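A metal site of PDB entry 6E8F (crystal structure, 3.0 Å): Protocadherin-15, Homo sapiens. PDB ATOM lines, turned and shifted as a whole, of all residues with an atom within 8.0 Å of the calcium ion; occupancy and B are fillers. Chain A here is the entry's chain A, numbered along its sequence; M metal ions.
OD1 of Asp 171 lies close to OD1 of Asn 129 (3.5 Å). The side-chain carboxylate of Asp 231 lies within hydrogen-bond range of the backbone NH of Val 233, 2.7 Å away. The side-chain carboxylate of Asp 231 sits close to the side-chain amide nitrogen of Asn 128, at 3.3 Å. The backbone NH of Gln 130 lies close to the side-chain amide nitrogen of Gln 234. The backbone NH (N) of Gln 234 is in hydrogen-bond range of the side-chain carboxylate (OD1) of Asp 231 (2.8 Å). OE1 of Gln 234 lies close to O of Asn 128. O of Lys 170 sits close to NE2 of Gln 130.
The nearest printed residue that does not touch the calcium ion is Gln 234 (4.2 Å).
The calcium ion is bound by OD2 of Asp 169 (2.1 Å), O of Gln 130 (2.3 Å), OD2 of Asp 171 (2.4 Å), OD2 of Asp 231 (2.5 Å) and OD1 of Asp 169 (2.5 Å). The calcium ion has five donor atoms within binding distance. Slightly farther from the calcium ion lies OD1 of Asn 128 (3.0 Å).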
ATOM      1  N   ASP A 126      20.836  -7.910  -0.553  1.00  0.00           N
ATOM      2  CA  ASP A 126      21.858  -8.927  -0.207  1.00  0.00           C
ATOM      3  C   ASP A 126      21.936  -8.979   1.325  1.00  0.00           C
ATOM      4  O   ASP A 126      22.269  -7.973   1.947  1.00  0.00           O
ATOM      5  CB  ASP A 126      23.218  -8.613  -0.850  1.00  0.00           C
ATOM      6  CG  ASP A 126      24.168  -9.805  -0.846  1.00  0.00           C
ATOM      7  OD1 ASP A 126      24.068 -10.645   0.074  1.00  0.00           O
ATOM      8  OD2 ASP A 126      25.018  -9.899  -1.771  1.00  0.00           O
ATOM      9  N   GLU A 127      21.576 -10.120   1.914  1.00  0.00           N
ATOM     10  CA  GLU A 127      21.543 -10.257   3.381  1.00  0.00           C
ATOM     11  C   GLU A 127      22.938 -10.716   3.841  1.00  0.00           C
ATOM     12  O   GLU A 127      23.629 -11.440   3.110  1.00  0.00           O
ATOM     13  CB  GLU A 127      20.384 -11.161   3.832  1.00  0.00           C
ATOM     14  CG  GLU A 127      20.566 -12.641   3.545  1.00  0.00           C
ATOM     15  CD  GLU A 127      19.592 -13.552   4.292  1.00  0.00           C
ATOM     16  OE1 GLU A 127      19.180 -14.594   3.710  1.00  0.00           O
ATOM     17  OE2 GLU A 127      19.275 -13.250   5.468  1.00  0.00           O
ATOM     18  N   ASN A 128      23.314 -10.273   5.056  1.00  0.00           N
ATOM     19  CA  ASN A 128      24.688 -10.273   5.560  1.00  0.00           C
ATOM     20  C   ASN A 128      25.080 -11.677   6.049  1.00  0.00           C
ATOM     21  O   ASN A 128      25.477 -11.856   7.195  1.00  0.00           O
ATOM     22  CB  ASN A 128      24.833  -9.222   6.669  1.00  0.00           C
ATOM     23  CG  ASN A 128      26.246  -8.677   6.813  1.00  0.00           C
ATOM     24  OD1 ASN A 128      26.753  -7.981   5.923  1.00  0.00           O
ATOM     25  ND2 ASN A 128      26.875  -8.959   7.947  1.00  0.00           N
ATOM     26  N   ASN A 129      24.996 -12.653   5.140  1.00  0.00           N
ATOM     27  CA  ASN A 129      25.143 -14.090   5.441  1.00  0.00           C
ATOM     28  C   ASN A 129      26.504 -14.623   4.977  1.00  0.00           C
ATOM     29  O   ASN A 129      26.728 -15.818   5.009  1.00  0.00           O
ATOM     30  CB  ASN A 129      24.023 -14.908   4.770  1.00  0.00           C
ATOM     31  CG  ASN A 129      24.196 -14.989   3.263  1.00  0.00           C
ATOM     32  OD1 ASN A 129      23.930 -14.034   2.543  1.00  0.00           O
ATOM     33  ND2 ASN A 129      24.672 -16.124   2.768  1.00  0.00           N
ATOM     34  N   GLN A 130      27.406 -13.747   4.523  1.00  0.00           N
ATOM     35  CA  GLN A 130      28.777 -14.151   4.138  1.00  0.00           C
ATOM     36  C   GLN A 130      29.794 -13.429   5.019  1.00  0.00           C
ATOM     37  O   GLN A 130      29.636 -12.225   5.314  1.00  0.00           O
ATOM     38  CB  GLN A 130      29.086 -13.824   2.670  1.00  0.00           C
ATOM     39  CG  GLN A 130      28.117 -14.436   1.681  1.00  0.00           C
ATOM     40  CD  GLN A 130      28.571 -14.201   0.260  1.00  0.00           C
ATOM     41  OE1 GLN A 130      29.436 -14.892  -0.264  1.00  0.00           O
ATOM     42  NE2 GLN A 130      27.976 -13.207  -0.391  1.00  0.00           N
ATOM     43  N   SER A 131      30.841 -14.154   5.426  1.00  0.00           N
ATOM     44  CA  SER A 131      31.848 -13.605   6.336  1.00  0.00           C
ATOM     45  C   SER A 131      33.002 -13.026   5.540  1.00  0.00           C
ATOM     46  O   SER A 131      33.352 -13.543   4.490  1.00  0.00           O
ATOM     47  CB  SER A 131      32.284 -14.627   7.375  1.00  0.00           C
ATOM     48  OG  SER A 131      33.071 -15.634   6.788  1.00  0.00           O
ATOM     49  N   PRO A 132      33.638 -11.915   5.975  1.00  0.00           N
ATOM     50  CA  PRO A 132      34.602 -11.215   5.138  1.00  0.00           C
ATOM     51  C   PRO A 132      35.912 -12.007   5.060  1.00  0.00           C
ATOM     52  O   PRO A 132      36.132 -12.980   5.821  1.00  0.00           O
ATOM     53  CB  PRO A 132      34.820  -9.848   5.794  1.00  0.00           C
ATOM     54  CG  PRO A 132      34.023  -9.891   7.093  1.00  0.00           C
ATOM     55  CD  PRO A 132      33.523 -11.306   7.307  1.00  0.00           C
ATOM     56  N   LEU A 168      37.467  -7.488   2.309  1.00  0.00           N
ATOM     57  CA  LEU A 168      36.212  -7.259   1.568  1.00  0.00           C
ATOM     58  C   LEU A 168      35.134  -8.241   2.068  1.00  0.00           C
ATOM     59  O   LEU A 168      35.443  -9.206   2.799  1.00  0.00           O
ATOM     60  CB  LEU A 168      36.450  -7.427   0.062  1.00  0.00           C
ATOM     61  CG  LEU A 168      37.730  -6.829  -0.523  1.00  0.00           C
ATOM     62  CD1 LEU A 168      38.086  -7.477  -1.844  1.00  0.00           C
ATOM     63  CD2 LEU A 168      37.626  -5.321  -0.706  1.00  0.00           C
ATOM     64  N   ASP A 169      33.888  -7.996   1.648  1.00  0.00           N
ATOM     65  CA  ASP A 169      32.713  -8.783   2.050  1.00  0.00           C
ATOM     66  C   ASP A 169      31.821  -8.946   0.804  1.00  0.00           C
ATOM     67  O   ASP A 169      31.368  -7.956   0.234  1.00  0.00           O
ATOM     68  CB  ASP A 169      31.990  -8.112   3.224  1.00  0.00           C
ATOM     69  CG  ASP A 169      30.919  -8.939   3.927  1.00  0.00           C
ATOM     70  OD1 ASP A 169      30.817 -10.147   3.681  1.00  0.00           O
ATOM     71  OD2 ASP A 169      30.174  -8.345   4.743  1.00  0.00           O
ATOM     72  N   LYS A 170      31.574 -10.196   0.403  1.00  0.00           N
ATOM     73  CA  LYS A 170      30.828 -10.456  -0.834  1.00  0.00           C
ATOM     74  C   LYS A 170      29.334 -10.108  -0.690  1.00  0.00           C
ATOM     75  O   LYS A 170      28.635 -10.092  -1.690  1.00  0.00           O
ATOM     76  CB  LYS A 170      31.052 -11.904  -1.290  1.00  0.00           C
ATOM     77  CG  LYS A 170      32.078 -12.030  -2.407  1.00  0.00           C
ATOM     78  CD  LYS A 170      32.782 -13.368  -2.444  1.00  0.00           C
ATOM     79  CE  LYS A 170      34.040 -13.328  -3.296  1.00  0.00           C
ATOM     80  NZ  LYS A 170      35.024 -14.354  -2.867  1.00  0.00           N
ATOM     81  N   ASP A 171      28.851  -9.804   0.519  1.00  0.00           N
ATOM     82  CA  ASP A 171      27.502  -9.245   0.711  1.00  0.00           C
ATOM     83  C   ASP A 171      27.485  -7.735   0.448  1.00  0.00           C
ATOM     84  O   ASP A 171      26.493  -7.072   0.747  1.00  0.00           O
ATOM     85  CB  ASP A 171      26.946  -9.476   2.122  1.00  0.00           C
ATOM     86  CG  ASP A 171      27.062 -10.896   2.635  1.00  0.00           C
ATOM     87  OD1 ASP A 171      26.495 -11.787   2.005  1.00  0.00           O
ATOM     88  OD2 ASP A 171      27.735 -11.088   3.653  1.00  0.00           O
ATOM     89  N   ILE A 172      28.588  -7.164  -0.058  1.00  0.00           N
ATOM     90  CA  ILE A 172      28.645  -5.722  -0.285  1.00  0.00           C
ATOM     91  C   ILE A 172      29.081  -5.447  -1.729  1.00  0.00           C
ATOM     92  O   ILE A 172      28.511  -4.583  -2.378  1.00  0.00           O
ATOM     93  CB  ILE A 172      29.584  -5.038   0.730  1.00  0.00           C
ATOM     94  CG1 ILE A 172      29.056  -5.169   2.161  1.00  0.00           C
ATOM     95  CG2 ILE A 172      29.821  -3.571   0.365  1.00  0.00           C
ATOM     96  CD1 ILE A 172      28.086  -4.087   2.579  1.00  0.00           C
ATOM     97  N   PRO A 185      33.332  -1.857   2.518  1.00  0.00           N
ATOM     98  CA  PRO A 185      32.479  -2.757   3.279  1.00  0.00           C
ATOM     99  C   PRO A 185      32.221  -2.393   4.757  1.00  0.00           C
ATOM    100  O   PRO A 185      31.522  -3.137   5.438  1.00  0.00           O
ATOM    101  CB  PRO A 185      33.199  -4.106   3.201  1.00  0.00           C
ATOM    102  CG  PRO A 185      34.631  -3.763   2.906  1.00  0.00           C
ATOM    103  CD  PRO A 185      34.550  -2.530   2.038  1.00  0.00           C
ATOM    104  N   LEU A 187      33.805  -2.435   7.768  1.00  0.00           N
ATOM    105  CA  LEU A 187      34.125  -3.593   8.559  1.00  0.00           C
ATOM    106  C   LEU A 187      34.886  -3.122   9.804  1.00  0.00           C
ATOM    107  O   LEU A 187      35.476  -2.039   9.774  1.00  0.00           O
ATOM    108  CB  LEU A 187      35.061  -4.491   7.744  1.00  0.00           C
ATOM    109  CG  LEU A 187      34.450  -5.384   6.694  1.00  0.00           C
ATOM    110  CD1 LEU A 187      35.535  -5.904   5.774  1.00  0.00           C
ATOM    111  CD2 LEU A 187      33.721  -6.538   7.337  1.00  0.00           C
ATOM    112  N   PHE A 230      35.284  -8.335  10.819  1.00  0.00           N
ATOM    113  CA  PHE A 230      33.919  -8.496  11.311  1.00  0.00           C
ATOM    114  C   PHE A 230      33.002  -7.519  10.586  1.00  0.00           C
ATOM    115  O   PHE A 230      33.337  -6.329  10.473  1.00  0.00           O
ATOM    116  CB  PHE A 230      33.907  -8.268  12.823  1.00  0.00           C
ATOM    117  CG  PHE A 230      32.563  -8.249  13.509  1.00  0.00           C
ATOM    118  CD1 PHE A 230      31.807  -9.401  13.649  1.00  0.00           C
ATOM    119  CD2 PHE A 230      32.124  -7.101  14.149  1.00  0.00           C
ATOM    120  CE1 PHE A 230      30.611  -9.385  14.349  1.00  0.00           C
ATOM    121  CE2 PHE A 230      30.922  -7.074  14.836  1.00  0.00           C
ATOM    122  CZ  PHE A 230      30.161  -8.221  14.926  1.00  0.00           C
ATOM    123  N   ASP A 231      31.851  -8.039  10.137  1.00  0.00           N
ATOM    124  CA  ASP A 231      30.864  -7.296   9.292  1.00  0.00           C
ATOM    125  C   ASP A 231      29.577  -6.914  10.043  1.00  0.00           C
ATOM    126  O   ASP A 231      28.685  -6.383   9.433  1.00  0.00           O
ATOM    127  CB  ASP A 231      30.454  -8.160   8.106  1.00  0.00           C
ATOM    128  CG  ASP A 231      29.845  -9.468   8.573  1.00  0.00           C
ATOM    129  OD1 ASP A 231      29.549  -9.553   9.795  1.00  0.00           O
ATOM    130  OD2 ASP A 231      29.708 -10.394   7.732  1.00  0.00           O
ATOM    131  N   GLY A 232      29.490  -7.163  11.364  1.00  0.00           N
ATOM    132  CA  GLY A 232      28.288  -6.939  12.143  1.00  0.00           C
ATOM    133  C   GLY A 232      27.646  -8.246  12.604  1.00  0.00           C
ATOM    134  O   GLY A 232      26.850  -8.253  13.532  1.00  0.00           O
ATOM    135  N   VAL A 233      28.018  -9.371  11.968  1.00  0.00           N
ATOM    136  CA  VAL A 233      27.356 -10.625  12.217  1.00  0.00           C
ATOM    137  C   VAL A 233      28.381 -11.767  12.315  1.00  0.00           C
ATOM    138  O   VAL A 233      28.290 -12.544  13.258  1.00  0.00           O
ATOM    139  CB  VAL A 233      26.295 -10.918  11.144  1.00  0.00           C
ATOM    140  CG1 VAL A 233      25.709 -12.324  11.264  1.00  0.00           C
ATOM    141  CG2 VAL A 233      25.189  -9.871  11.127  1.00  0.00           C
ATOM    142  N   GLN A 234      29.269 -11.924  11.311  1.00  0.00           N
ATOM    143  CA  GLN A 234      30.281 -12.995  11.314  1.00  0.00           C
ATOM    144  C   GLN A 234      31.681 -12.428  11.076  1.00  0.00           C
ATOM    145  O   GLN A 234      31.833 -11.299  10.553  1.00  0.00           O
ATOM    146  CB  GLN A 234      30.119 -14.041  10.209  1.00  0.00           C
ATOM    147  CG  GLN A 234      28.695 -14.444   9.907  1.00  0.00           C
ATOM    148  CD  GLN A 234      28.159 -13.722   8.701  1.00  0.00           C
ATOM    149  OE1 GLN A 234      28.171 -12.488   8.627  1.00  0.00           O
ATOM    150  NE2 GLN A 234      27.692 -14.493   7.746  1.00  0.00           N
ATOM    151  N   GLU A 235      32.675 -13.286  11.343  1.00  0.00           N
ATOM    152  CA  GLU A 235      34.073 -12.937  11.269  1.00  0.00           C
ATOM    153  C   GLU A 235      34.792 -13.700  10.151  1.00  0.00           C
ATOM    154  O   GLU A 235      34.410 -14.811   9.769  1.00  0.00           O
ATOM    155  CB  GLU A 235      34.767 -13.305  12.572  1.00  0.00           C
ATOM    156  CG  GLU A 235      34.124 -12.690  13.788  1.00  0.00           C
ATOM    157  CD  GLU A 235      34.957 -12.878  15.044  1.00  0.00           C
ATOM    158  OE1 GLU A 235      35.337 -14.033  15.346  1.00  0.00           O
ATOM    159  OE2 GLU A 235      35.231 -11.851  15.697  1.00  0.00           O
HETATM  160 CA    CA M   1      28.951  -9.980   5.404  1.00  0.00          CA
